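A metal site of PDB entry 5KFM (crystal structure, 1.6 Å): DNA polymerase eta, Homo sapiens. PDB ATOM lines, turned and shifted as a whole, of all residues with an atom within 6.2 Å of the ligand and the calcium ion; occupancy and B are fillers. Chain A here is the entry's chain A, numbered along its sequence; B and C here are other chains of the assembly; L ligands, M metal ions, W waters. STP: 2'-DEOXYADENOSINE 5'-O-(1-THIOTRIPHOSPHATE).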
ATOM      1  N   ASP A  16      23.362  15.412  22.184  1.00  0.00           N
ATOM      2  CA  ASP A  16      23.650  14.012  22.488  1.00  0.00           C
ATOM      3  C   ASP A  16      22.574  13.109  21.847  1.00  0.00           C
ATOM      4  O   ASP A  16      21.418  13.126  22.292  1.00  0.00           O
ATOM      5  CB  ASP A  16      23.670  13.841  24.020  1.00  0.00           C
ATOM      6  CG  ASP A  16      24.046  12.451  24.477  1.00  0.00           C
ATOM      7  OD1 ASP A  16      24.233  12.292  25.709  1.00  0.00           O
ATOM      8  OD2 ASP A  16      24.142  11.535  23.651  1.00  0.00           O
ATOM      9  N   MET A  17      22.925  12.343  20.843  1.00  0.00           N
ATOM     10  CA  MET A  17      21.903  11.554  20.171  1.00  0.00           C
ATOM     11  C   MET A  17      21.288  10.515  21.103  1.00  0.00           C
ATOM     12  O   MET A  17      21.950  10.003  21.895  1.00  0.00           O
ATOM     13  CB  MET A  17      22.450  10.834  18.935  1.00  0.00           C
ATOM     14  CG  MET A  17      23.196  11.723  17.966  1.00  0.00           C
ATOM     15  SD  MET A  17      22.190  13.053  17.237  1.00  0.00           S
ATOM     16  CE  MET A  17      21.059  12.102  16.269  1.00  0.00           C
ATOM     17  N   ASP A  18      20.003  10.239  20.959  1.00  0.00           N
ATOM     18  CA  ASP A  18      19.391   9.257  21.818  1.00  0.00           C
ATOM     19  C   ASP A  18      19.661   7.847  21.293  1.00  0.00           C
ATOM     20  O   ASP A  18      19.627   7.654  20.116  1.00  0.00           O
ATOM     21  CB  ASP A  18      17.896   9.438  21.874  1.00  0.00           C
ATOM     22  CG  ASP A  18      17.480  10.778  22.424  1.00  0.00           C
ATOM     23  OD1 ASP A  18      18.115  11.279  23.266  1.00  0.00           O
ATOM     24  OD2 ASP A  18      16.465  11.252  22.023  1.00  0.00           O
ATOM     25  N   CYS A  19      20.053   6.971  22.193  1.00  0.00           N
ATOM     26  CA  CYS A  19      20.248   5.562  21.929  1.00  0.00           C
ATOM     27  C   CYS A  19      20.864   5.318  20.551  1.00  0.00           C
ATOM     28  O   CYS A  19      20.299   4.688  19.763  1.00  0.00           O
ATOM     29  CB  CYS A  19      19.086   4.658  22.254  1.00  0.00           C
ATOM     30  SG  CYS A  19      17.519   4.986  21.464  1.00  0.00           S
ATOM     31  N   PHE A  20      21.970   5.976  20.280  1.00  0.00           N
ATOM     32  CA  PHE A  20      22.341   6.239  18.904  1.00  0.00           C
ATOM     33  C   PHE A  20      22.548   5.029  18.025  1.00  0.00           C
ATOM     34  O   PHE A  20      21.974   4.992  17.026  1.00  0.00           O
ATOM     35  CB  PHE A  20      23.632   7.038  18.897  1.00  0.00           C
ATOM     36  CG  PHE A  20      24.097   7.447  17.566  1.00  0.00           C
ATOM     37  CD1 PHE A  20      23.278   8.075  16.716  1.00  0.00           C
ATOM     38  CD2 PHE A  20      25.371   7.179  17.155  1.00  0.00           C
ATOM     39  CE1 PHE A  20      23.690   8.464  15.478  1.00  0.00           C
ATOM     40  CE2 PHE A  20      25.793   7.562  15.905  1.00  0.00           C
ATOM     41  CZ  PHE A  20      24.953   8.220  15.094  1.00  0.00           C
ATOM     42  N   PHE A  21      23.303   4.022  18.432  1.00  0.00           N
ATOM     43  CA  PHE A  21      23.476   2.877  17.519  1.00  0.00           C
ATOM     44  C   PHE A  21      22.127   2.186  17.267  1.00  0.00           C
ATOM     45  O   PHE A  21      21.885   1.673  16.176  1.00  0.00           O
ATOM     46  CB  PHE A  21      24.478   1.834  18.043  1.00  0.00           C
ATOM     47  CG  PHE A  21      25.927   2.280  18.048  1.00  0.00           C
ATOM     48  CD1 PHE A  21      26.301   3.597  17.830  1.00  0.00           C
ATOM     49  CD2 PHE A  21      26.934   1.354  18.279  1.00  0.00           C
ATOM     50  CE1 PHE A  21      27.629   3.985  17.828  1.00  0.00           C
ATOM     51  CE2 PHE A  21      28.270   1.735  18.278  1.00  0.00           C
ATOM     52  CZ  PHE A  21      28.614   3.031  18.063  1.00  0.00           C
ATOM     53  N   VAL A  22      21.267   2.164  18.292  1.00  0.00           N
ATOM     54  CA  VAL A  22      19.922   1.642  18.123  1.00  0.00           C
ATOM     55  C   VAL A  22      19.169   2.414  17.051  1.00  0.00           C
ATOM     56  O   VAL A  22      18.563   1.808  16.143  1.00  0.00           O
ATOM     57  CB  VAL A  22      19.125   1.673  19.440  1.00  0.00           C
ATOM     58  CG1 VAL A  22      17.615   1.543  19.164  1.00  0.00           C
ATOM     59  CG2 VAL A  22      19.570   0.535  20.329  1.00  0.00           C
ATOM     60  N   GLN A  41      27.459  -6.838  19.940  1.00  0.00           N
ATOM     61  CA  GLN A  41      28.580  -7.205  19.084  1.00  0.00           C
ATOM     62  C   GLN A  41      29.010  -8.610  19.435  1.00  0.00           C
ATOM     63  O   GLN A  41      29.102  -8.968  20.608  1.00  0.00           O
ATOM     64  CB  GLN A  41      29.738  -6.226  19.200  1.00  0.00           C
ATOM     65  CG  GLN A  41      30.154  -5.877  20.594  1.00  0.00           C
ATOM     66  CD  GLN A  41      31.185  -4.767  20.612  1.00  0.00           C
ATOM     67  OE1 GLN A  41      31.481  -4.162  19.570  1.00  0.00           O
ATOM     68  NE2 GLN A  41      31.742  -4.490  21.783  1.00  0.00           N
ATOM     69  N   ILE A  51      25.835  -3.089  23.487  1.00  0.00           N
ATOM     70  CA  ILE A  51      26.468  -1.778  23.559  1.00  0.00           C
ATOM     71  C   ILE A  51      25.495  -0.609  23.421  1.00  0.00           C
ATOM     72  O   ILE A  51      25.886   0.528  23.628  1.00  0.00           O
ATOM     73  CB  ILE A  51      27.584  -1.609  22.507  1.00  0.00           C
ATOM     74  CG1 ILE A  51      27.056  -1.781  21.081  1.00  0.00           C
ATOM     75  CG2 ILE A  51      28.751  -2.599  22.794  1.00  0.00           C
ATOM     76  CD1 ILE A  51      28.123  -1.512  20.029  1.00  0.00           C
ATOM     77  N   ALA A  52      24.237  -0.888  23.066  1.00  0.00           N
ATOM     78  CA  ALA A  52      23.216   0.179  22.988  1.00  0.00           C
ATOM     79  C   ALA A  52      21.829  -0.394  23.200  1.00  0.00           C
ATOM     80  O   ALA A  52      21.550  -1.521  22.800  1.00  0.00           O
ATOM     81  CB  ALA A  52      23.297   0.927  21.638  1.00  0.00           C
ATOM     82  N   VAL A  53      20.957   0.388  23.838  1.00  0.00           N
ATOM     83  CA  VAL A  53      19.642  -0.081  24.285  1.00  0.00           C
ATOM     84  C   VAL A  53      18.559   0.957  24.043  1.00  0.00           C
ATOM     85  O   VAL A  53      18.693   2.113  24.460  1.00  0.00           O
ATOM     86  CB  VAL A  53      19.654  -0.397  25.811  1.00  0.00           C
ATOM     87  CG1 VAL A  53      18.394  -1.100  26.212  1.00  0.00           C
ATOM     88  CG2 VAL A  53      20.864  -1.266  26.173  1.00  0.00           C
ATOM     89  N   TYR A  55      14.927   2.833  24.552  1.00  0.00           N
ATOM     90  CA  TYR A  55      14.275   3.204  25.796  1.00  0.00           C
ATOM     91  C   TYR A  55      13.169   2.218  26.172  1.00  0.00           C
ATOM     92  O   TYR A  55      12.962   1.952  27.355  1.00  0.00           O
ATOM     93  CB  TYR A  55      13.770   4.661  25.720  1.00  0.00           C
ATOM     94  CG  TYR A  55      14.923   5.630  25.913  1.00  0.00           C
ATOM     95  CD1 TYR A  55      15.800   5.918  24.865  1.00  0.00           C
ATOM     96  CD2 TYR A  55      15.192   6.191  27.156  1.00  0.00           C
ATOM     97  CE1 TYR A  55      16.888   6.768  25.045  1.00  0.00           C
ATOM     98  CE2 TYR A  55      16.270   7.047  27.349  1.00  0.00           C
ATOM     99  CZ  TYR A  55      17.124   7.335  26.298  1.00  0.00           C
ATOM    100  OH  TYR A  55      18.198   8.168  26.484  1.00  0.00           O
ATOM    101  N   ARG A  58      15.023  -0.391  27.945  1.00  0.00           N
ATOM    102  CA  ARG A  58      15.530   0.057  29.235  1.00  0.00           C
ATOM    103  C   ARG A  58      14.463  -0.107  30.314  1.00  0.00           C
ATOM    104  O   ARG A  58      14.804  -0.342  31.481  1.00  0.00           O
ATOM    105  CB  ARG A  58      15.980   1.517  29.166  1.00  0.00           C
ATOM    106  CG  ARG A  58      17.189   1.719  28.275  1.00  0.00           C
ATOM    107  CD  ARG A  58      17.639   3.162  28.207  1.00  0.00           C
ATOM    108  NE  ARG A  58      18.497   3.339  27.051  1.00  0.00           N
ATOM    109  CZ  ARG A  58      19.296   4.369  26.834  1.00  0.00           C
ATOM    110  NH1 ARG A  58      19.346   5.366  27.707  1.00  0.00           N
ATOM    111  NH2 ARG A  58      20.037   4.400  25.723  1.00  0.00           N
ATOM    112  N   ARG A  64      23.580  -1.447  28.810  1.00  0.00           N
ATOM    113  CA  ARG A  64      24.897  -1.662  28.205  1.00  0.00           C
ATOM    114  C   ARG A  64      25.721  -2.589  29.096  1.00  0.00           C
ATOM    115  O   ARG A  64      25.507  -2.611  30.310  1.00  0.00           O
ATOM    116  CB  ARG A  64      25.612  -0.329  27.993  1.00  0.00           C
ATOM    117  CG  ARG A  64      27.077  -0.407  27.632  1.00  0.00           C
ATOM    118  CD  ARG A  64      27.621   0.959  27.285  1.00  0.00           C
ATOM    119  NE  ARG A  64      26.876   1.534  26.160  1.00  0.00           N
ATOM    120  CZ  ARG A  64      26.071   2.584  26.253  1.00  0.00           C
ATOM    121  NH1 ARG A  64      25.917   3.206  27.413  1.00  0.00           N
ATOM    122  NH2 ARG A  64      25.417   3.005  25.178  1.00  0.00           N
ATOM    123  N   SER A 116      32.316  12.935  21.108  1.00  0.00           N
ATOM    124  CA  SER A 116      32.317  11.500  21.006  1.00  0.00           C
ATOM    125  C   SER A 116      31.621  11.152  19.711  1.00  0.00           C
ATOM    126  O   SER A 116      31.334  12.031  18.896  1.00  0.00           O
ATOM    127  CB  SER A 116      31.586  10.851  22.186  1.00  0.00           C
ATOM    128  OG  SER A 116      30.200  11.152  22.126  1.00  0.00           O
ATOM    129  N   ILE A 117      31.332   9.867  19.505  1.00  0.00           N
ATOM    130  CA  ILE A 117      30.717   9.452  18.265  1.00  0.00           C
ATOM    131  C   ILE A 117      29.332  10.087  18.042  1.00  0.00           C
ATOM    132  O   ILE A 117      28.915  10.279  16.916  1.00  0.00           O
ATOM    133  CB  ILE A 117      30.607   7.913  18.200  1.00  0.00           C
ATOM    134  CG1 ILE A 117      30.348   7.477  16.749  1.00  0.00           C
ATOM    135  CG2 ILE A 117      29.558   7.395  19.196  1.00  0.00           C
ATOM    136  CD1 ILE A 117      30.647   6.017  16.464  1.00  0.00           C
ATOM    137  N   ASP A 118      28.649  10.486  19.117  1.00  0.00           N
ATOM    138  CA  ASP A 118      27.286  10.993  18.942  1.00  0.00           C
ATOM    139  C   ASP A 118      26.968  12.218  19.792  1.00  0.00           C
ATOM    140  O   ASP A 118      25.796  12.499  20.079  1.00  0.00           O
ATOM    141  CB  ASP A 118      26.283   9.880  19.247  1.00  0.00           C
ATOM    142  CG  ASP A 118      26.092   9.659  20.739  1.00  0.00           C
ATOM    143  OD1 ASP A 118      24.985   9.285  21.139  1.00  0.00           O
ATOM    144  OD2 ASP A 118      27.047   9.869  21.512  1.00  0.00           O
ATOM    145  N   GLU A 119      28.021  12.917  20.198  1.00  0.00           N
ATOM    146  CA  GLU A 119      27.915  14.105  21.047  1.00  0.00           C
ATOM    147  C   GLU A 119      28.766  15.220  20.487  1.00  0.00           C
ATOM    148  O   GLU A 119      29.887  14.974  20.021  1.00  0.00           O
ATOM    149  CB  GLU A 119      28.381  13.834  22.480  1.00  0.00           C
ATOM    150  CG  GLU A 119      27.600  12.782  23.255  1.00  0.00           C
ATOM    151  CD  GLU A 119      28.179  12.570  24.659  1.00  0.00           C
ATOM    152  OE1 GLU A 119      29.279  13.102  24.903  1.00  0.00           O
ATOM    153  OE2 GLU A 119      27.537  11.889  25.488  1.00  0.00           O
ATOM    154  N   LYS A 227      26.306  19.743  29.410  1.00  0.00           N
ATOM    155  CA  LYS A 227      26.298  18.287  29.435  1.00  0.00           C
ATOM    156  C   LYS A 227      25.352  17.772  30.529  1.00  0.00           C
ATOM    157  O   LYS A 227      24.532  16.893  30.277  1.00  0.00           O
ATOM    158  CB  LYS A 227      27.713  17.755  29.646  1.00  0.00           C
ATOM    159  CG  LYS A 227      27.782  16.253  29.861  1.00  0.00           C
ATOM    160  CD  LYS A 227      27.186  15.498  28.700  1.00  0.00           C
ATOM    161  CE  LYS A 227      27.352  13.998  28.870  1.00  0.00           C
ATOM    162  NZ  LYS A 227      26.556  13.258  27.855  1.00  0.00           N
ATOM    163  N   LYS A 234      16.406  13.551  28.889  1.00  0.00           N
ATOM    164  CA  LYS A 234      16.484  12.523  27.848  1.00  0.00           C
ATOM    165  C   LYS A 234      15.280  11.589  27.947  1.00  0.00           C
ATOM    166  O   LYS A 234      14.850  11.285  29.060  1.00  0.00           O
ATOM    167  CB  LYS A 234      17.762  11.684  27.983  1.00  0.00           C
ATOM    168  CG  LYS A 234      18.927  12.119  27.147  1.00  0.00           C
ATOM    169  CD  LYS A 234      19.969  11.001  26.986  1.00  0.00           C
ATOM    170  CE  LYS A 234      21.054  11.420  25.997  1.00  0.00           C
ATOM    171  NZ  LYS A 234      20.600  11.326  24.558  1.00  0.00           N
ATOM    172  N   PRO A 235      14.759  11.086  26.814  1.00  0.00           N
ATOM    173  CA  PRO A 235      15.161  11.387  25.433  1.00  0.00           C
ATOM    174  C   PRO A 235      14.270  12.395  24.739  1.00  0.00           C
ATOM    175  O   PRO A 235      13.189  12.733  25.237  1.00  0.00           O
ATOM    176  CB  PRO A 235      15.005  10.038  24.746  1.00  0.00           C
ATOM    177  CG  PRO A 235      13.747   9.501  25.409  1.00  0.00           C
ATOM    178  CD  PRO A 235      13.864   9.920  26.870  1.00  0.00           C
ATOM    179  P    DT B   3      33.334 -10.122  32.039  1.00  0.00           P
ATOM    180  OP1  DT B   3      34.321 -10.430  33.090  1.00  0.00           O
ATOM    181  OP2  DT B   3      31.887 -10.322  32.287  1.00  0.00           O
ATOM    182  O5'  DT B   3      33.549  -8.611  31.569  1.00  0.00           O
ATOM    183  C5'  DT B   3      32.541  -7.928  30.830  1.00  0.00           C
ATOM    184  C4'  DT B   3      32.692  -8.185  29.349  1.00  0.00           C
ATOM    185  O4'  DT B   3      31.736  -7.365  28.628  1.00  0.00           O
ATOM    186  C3'  DT B   3      34.059  -7.852  28.769  1.00  0.00           C
ATOM    187  O3'  DT B   3      34.348  -8.698  27.680  1.00  0.00           O
ATOM    188  C2'  DT B   3      33.859  -6.418  28.304  1.00  0.00           C
ATOM    189  C1'  DT B   3      32.437  -6.462  27.789  1.00  0.00           C
ATOM    190  N1   DT B   3      31.753  -5.146  27.849  1.00  0.00           N
ATOM    191  C2   DT B   3      30.986  -4.737  26.782  1.00  0.00           C
ATOM    192  O2   DT B   3      30.813  -5.408  25.781  1.00  0.00           O
ATOM    193  N3   DT B   3      30.402  -3.504  26.942  1.00  0.00           N
ATOM    194  C4   DT B   3      30.521  -2.657  28.032  1.00  0.00           C
ATOM    195  O4   DT B   3      29.953  -1.571  28.083  1.00  0.00           O
ATOM    196  C5   DT B   3      31.349  -3.149  29.109  1.00  0.00           C
ATOM    197  C7   DT B   3      31.551  -2.332  30.346  1.00  0.00           C
ATOM    198  C6   DT B   3      31.911  -4.357  28.967  1.00  0.00           C
ATOM    199  P    DT B   4      35.647  -8.449  26.778  1.00  0.00           P
ATOM    200  OP1  DT B   4      35.991  -9.736  26.125  1.00  0.00           O
ATOM    201  OP2  DT B   4      36.652  -7.720  27.599  1.00  0.00           O
ATOM    202  O5'  DT B   4      35.154  -7.450  25.643  1.00  0.00           O
ATOM    203  C5'  DT B   4      34.311  -7.939  24.617  1.00  0.00           C
ATOM    204  C4'  DT B   4      34.292  -6.995  23.429  1.00  0.00           C
ATOM    205  O4'  DT B   4      33.649  -5.752  23.795  1.00  0.00           O
ATOM    206  C3'  DT B   4      35.650  -6.604  22.875  1.00  0.00           C
ATOM    207  O3'  DT B   4      35.515  -6.444  21.471  1.00  0.00           O
ATOM    208  C2'  DT B   4      35.923  -5.265  23.584  1.00  0.00           C
ATOM    209  C1'  DT B   4      34.522  -4.662  23.566  1.00  0.00           C
ATOM    210  N1   DT B   4      34.218  -3.649  24.600  1.00  0.00           N
ATOM    211  C2   DT B   4      33.350  -2.643  24.272  1.00  0.00           C
ATOM    212  O2   DT B   4      32.888  -2.524  23.155  1.00  0.00           O
ATOM    213  N3   DT B   4      33.061  -1.780  25.267  1.00  0.00           N
ATOM    214  C4   DT B   4      33.520  -1.804  26.567  1.00  0.00           C
ATOM    215  O4   DT B   4      33.182  -0.972  27.393  1.00  0.00           O
ATOM    216  C5   DT B   4      34.410  -2.915  26.885  1.00  0.00           C
ATOM    217  C7   DT B   4      34.986  -3.035  28.272  1.00  0.00           C
ATOM    218  C6   DT B   4      34.710  -3.778  25.898  1.00  0.00           C
ATOM    219  P    DA B   5      36.762  -6.054  20.525  1.00  0.00           P
ATOM    220  OP1  DA B   5      36.656  -6.875  19.314  1.00  0.00           O
ATOM    221  OP2  DA B   5      38.025  -6.018  21.320  1.00  0.00           O
ATOM    222  O5'  DA B   5      36.455  -4.545  20.145  1.00  0.00           O
ATOM    223  C5'  DA B   5      35.347  -4.241  19.300  1.00  0.00           C
ATOM    224  C4'  DA B   5      35.316  -2.758  19.070  1.00  0.00           C
ATOM    225  O4'  DA B   5      34.957  -2.121  20.325  1.00  0.00           O
ATOM    226  C3'  DA B   5      36.654  -2.139  18.644  1.00  0.00           C
ATOM    227  O3'  DA B   5      36.421  -1.179  17.621  1.00  0.00           O
ATOM    228  C2'  DA B   5      37.156  -1.483  19.937  1.00  0.00           C
ATOM    229  C1'  DA B   5      35.847  -1.043  20.540  1.00  0.00           C
ATOM    230  N9   DA B   5      35.906  -0.755  21.968  1.00  0.00           N
ATOM    231  C8   DA B   5      36.598  -1.446  22.924  1.00  0.00           C
ATOM    232  N7   DA B   5      36.437  -0.956  24.135  1.00  0.00           N
ATOM    233  C5   DA B   5      35.578   0.121  23.949  1.00  0.00           C
ATOM    234  C6   DA B   5      35.025   1.050  24.839  1.00  0.00           C
ATOM    235  N6   DA B   5      35.269   1.046  26.153  1.00  0.00           N
ATOM    236  N1   DA B   5      34.207   1.988  24.326  1.00  0.00           N
ATOM    237  C2   DA B   5      33.964   1.992  23.011  1.00  0.00           C
ATOM    238  N3   DA B   5      34.440   1.169  22.075  1.00  0.00           N
ATOM    239  C4   DA B   5      35.242   0.250  22.621  1.00  0.00           C
ATOM    240  P    DT C   8      29.955   9.392  29.105  1.00  0.00           P
ATOM    241  OP1  DT C   8      28.830  10.340  29.287  1.00  0.00           O
ATOM    242  OP2  DT C   8      29.957   8.096  29.835  1.00  0.00           O
ATOM    243  O5'  DT C   8      30.225   8.998  27.557  1.00  0.00           O
ATOM    244  C5'  DT C   8      30.006   9.940  26.514  1.00  0.00           C
ATOM    245  C4'  DT C   8      30.341   9.349  25.142  1.00  0.00           C
ATOM    246  O4'  DT C   8      31.483   8.473  25.231  1.00  0.00           O
ATOM    247  C3'  DT C   8      29.228   8.539  24.458  1.00  0.00           C
ATOM    248  O3'  DT C   8      29.136   8.913  23.100  1.00  0.00           O
ATOM    249  C2'  DT C   8      29.682   7.097  24.613  1.00  0.00           C
ATOM    250  C1'  DT C   8      31.192   7.229  24.632  1.00  0.00           C
ATOM    251  N1   DT C   8      31.852   6.150  25.406  1.00  0.00           N
ATOM    252  C2   DT C   8      32.429   5.096  24.735  1.00  0.00           C
ATOM    253  O2   DT C   8      32.432   4.994  23.525  1.00  0.00           O
ATOM    254  N3   DT C   8      33.017   4.159  25.540  1.00  0.00           N
ATOM    255  C4   DT C   8      33.063   4.158  26.914  1.00  0.00           C
ATOM    256  O4   DT C   8      33.620   3.266  27.550  1.00  0.00           O
ATOM    257  C5   DT C   8      32.425   5.278  27.562  1.00  0.00           C
ATOM    258  C7   DT C   8      32.422   5.384  29.064  1.00  0.00           C
ATOM    259  C6   DT C   8      31.858   6.214  26.788  1.00  0.00           C
HETATM  260  PG  STP L   1      21.580   7.711  25.411  1.00  0.00           P
HETATM  261  O1G STP L   1      22.540   8.777  24.972  1.00  0.00           O
HETATM  262  O2G STP L   1      20.190   7.978  24.923  1.00  0.00           O
HETATM  263  O3G STP L   1      21.628   7.457  26.926  1.00  0.00           O
HETATM  264  PB  STP L   1      23.294   6.069  23.833  1.00  0.00           P
HETATM  265  O1B STP L   1      23.359   7.104  22.725  1.00  0.00           O
HETATM  266  O2B STP L   1      23.176   4.685  23.223  1.00  0.00           O
HETATM  267  O3B STP L   1      22.000   6.294  24.770  1.00  0.00           O
HETATM  268  PA  STP L   1      25.873   6.935  24.788  1.00  0.00           P
HETATM  269  S1A STP L   1      26.699   6.677  26.530  1.00  0.00           S
HETATM  270  O2A STP L   1      25.568   8.352  24.424  1.00  0.00           O
HETATM  271  O3A STP L   1      24.531   6.063  24.846  1.00  0.00           O
HETATM  272  O5' STP L   1      26.803   6.260  23.692  1.00  0.00           O
HETATM  273  C5' STP L   1      26.628   6.510  22.332  1.00  0.00           C
HETATM  274  C4' STP L   1      26.928   5.279  21.494  1.00  0.00           C
HETATM  275  O4' STP L   1      28.277   4.929  21.729  1.00  0.00           O
HETATM  276  C3' STP L   1      26.107   4.155  21.887  1.00  0.00           C
HETATM  277  O3' STP L   1      24.871   4.112  21.139  1.00  0.00           O
HETATM  278  C2' STP L   1      26.947   2.986  21.616  1.00  0.00           C
HETATM  279  C1' STP L   1      28.329   3.484  21.840  1.00  0.00           C
HETATM  280  N9  STP L   1      28.831   3.152  23.129  1.00  0.00           N
HETATM  281  C8  STP L   1      28.584   3.772  24.305  1.00  0.00           C
HETATM  282  N7  STP L   1      29.242   3.176  25.298  1.00  0.00           N
HETATM  283  C5  STP L   1      29.944   2.148  24.793  1.00  0.00           C
HETATM  284  C6  STP L   1      30.807   1.185  25.305  1.00  0.00           C
HETATM  285  N6  STP L   1      31.125   1.127  26.694  1.00  0.00           N
HETATM  286  N1  STP L   1      31.327   0.305  24.460  1.00  0.00           N
HETATM  287  C2  STP L   1      31.071   0.292  23.137  1.00  0.00           C
HETATM  288  N3  STP L   1      30.248   1.218  22.595  1.00  0.00           N
HETATM  289  C4  STP L   1      29.692   2.128  23.407  1.00  0.00           C
HETATM  290 CA    CA M   1      23.840   9.356  23.159  1.00  0.00          CA
HETATM  291  O   HOH W   1      25.276   9.998  26.574  1.00  0.00           O
HETATM  292  O   HOH W   2      30.464   2.150  29.586  1.00  0.00           O
HETATM  293  O   HOH W   3      23.229   5.687  27.967  1.00  0.00           O
HETATM  294  O   HOH W   4      31.138   1.229  19.864  1.00  0.00           O
HETATM  295  O   HOH W   5      23.546   9.018  28.261  1.00  0.00           O
HETATM  296  O   HOH W   6      31.303   5.183  21.396  1.00  0.00           O
HETATM  297  O   HOH W   7      29.128   3.628  28.127  1.00  0.00           O
HETATM  298  O   HOH W   8      22.178   2.740  24.892  1.00  0.00           O
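An oxygen (O3G) of the ligand is in salt-bridge range of the guanidinium group (NH1) of Arg 58. O4 of DT 8 of chain C is in hydrogen-bond range of a nitrogen (N6) of the ligand, at 3.4 Å. N6 of the ligand sits at hydrogen-bond distance from O4 of DT 3 of chain B, at 3.3 Å. NZ of Lys 234 is in salt-bridge range of O2G of the ligand (3.4 Å). O4 of DT 4 of chain B sits at hydrogen-bond distance from N6 of the ligand (3.0 Å). O2G of the ligand sits at hydrogen-bond distance from N of Cys 19, at 2.9 Å. An oxygen (O2B) of the ligand lies within hydrogen-bond range of the backbone NH (N) of Phe 20, 3.4 Å away. The side-chain hydroxyl of Tyr 55 sits at hydrogen-bond distance from an oxygen (O2G) of the ligand, at 2.5 Å. The backbone NH of Phe 21 sits at hydrogen-bond distance from an oxygen (O3') of the ligand, at 3.1 Å. O2B of the ligand lies within salt-bridge range of NH2 of Arg 64 (3.4 Å).
OD1 of Asp 16 lies within salt-bridge range of NZ of Lys 227 (3.3 Å). NZ of Lys 234 lies within salt-bridge range of OD1 of Asp 18, 2.8 Å away. The backbone NH (N) of Asp 118 sits close to the side-chain hydroxyl (OG) of Ser 116 (3.5 Å). OH of Tyr 55 is in hydrogen-bond range of NH1 of Arg 58 (3.3 Å). O2 of DT 4 of chain B is in hydrogen-bond range of the side-chain amide nitrogen (NE2) of Gln 41 (2.7 Å). The side-chain amino group (NZ) of Lys 234 lies close to the backbone carbonyl oxygen (O) of Met 17 (3.3 Å). The side-chain carboxylate (OD1) of Asp 16 lies within salt-bridge range of the side-chain amino group (NZ) of Lys 234 (3.9 Å). OP1 of DT 8 of chain C is in salt-bridge range of the side-chain amino group (NZ) of Lys 227, at 3.97 Å.
N1 of the ligand lies close to N1 of DA 5 of chain B (3.3 Å). Residues that only touch the ligand: Ile 51 (3.3 Å), Asp 18 (3.5 Å), Ala 52 (3.6 Å) and Ile 117 (3.8 Å). Hydrophobic or aromatic side chains within 4 Å of the ligand: Phe 20, Phe 21, Ile 51, Ala 52, Tyr 55 and Ile 117. Of the 25 residues printed, 18 come within 4 Å of the ligand.
The nearest printed residue that does not touch the calcium ion is Lys 234 (4.04 Å).
OD2 of Asp 16 binds the calcium ion, at 2.3 Å. The calcium ion is bound by an oxygen (O1G) of the ligand, at 2.3 Å. The side-chain carboxylate (OD1) of Asp 118 is bound to the calcium ion, 2.3 Å away. O1B of the ligand binds the calcium ion, at 2.3 Å. O of Met 17 binds the calcium ion, 2.4 Å away. The calcium ion is bound by O2A of the ligand, 2.4 Å away. The calcium ion has six donor atoms within binding distance.
Water W7 lies within hydrogen-bond range of a nitrogen (N7) of the ligand and the guanidinium group (NH1) of Arg 64. Water W6 bridges O2 of DT 8 of chain C (2.4 Å) and O4' of the ligand (3.1 Å).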
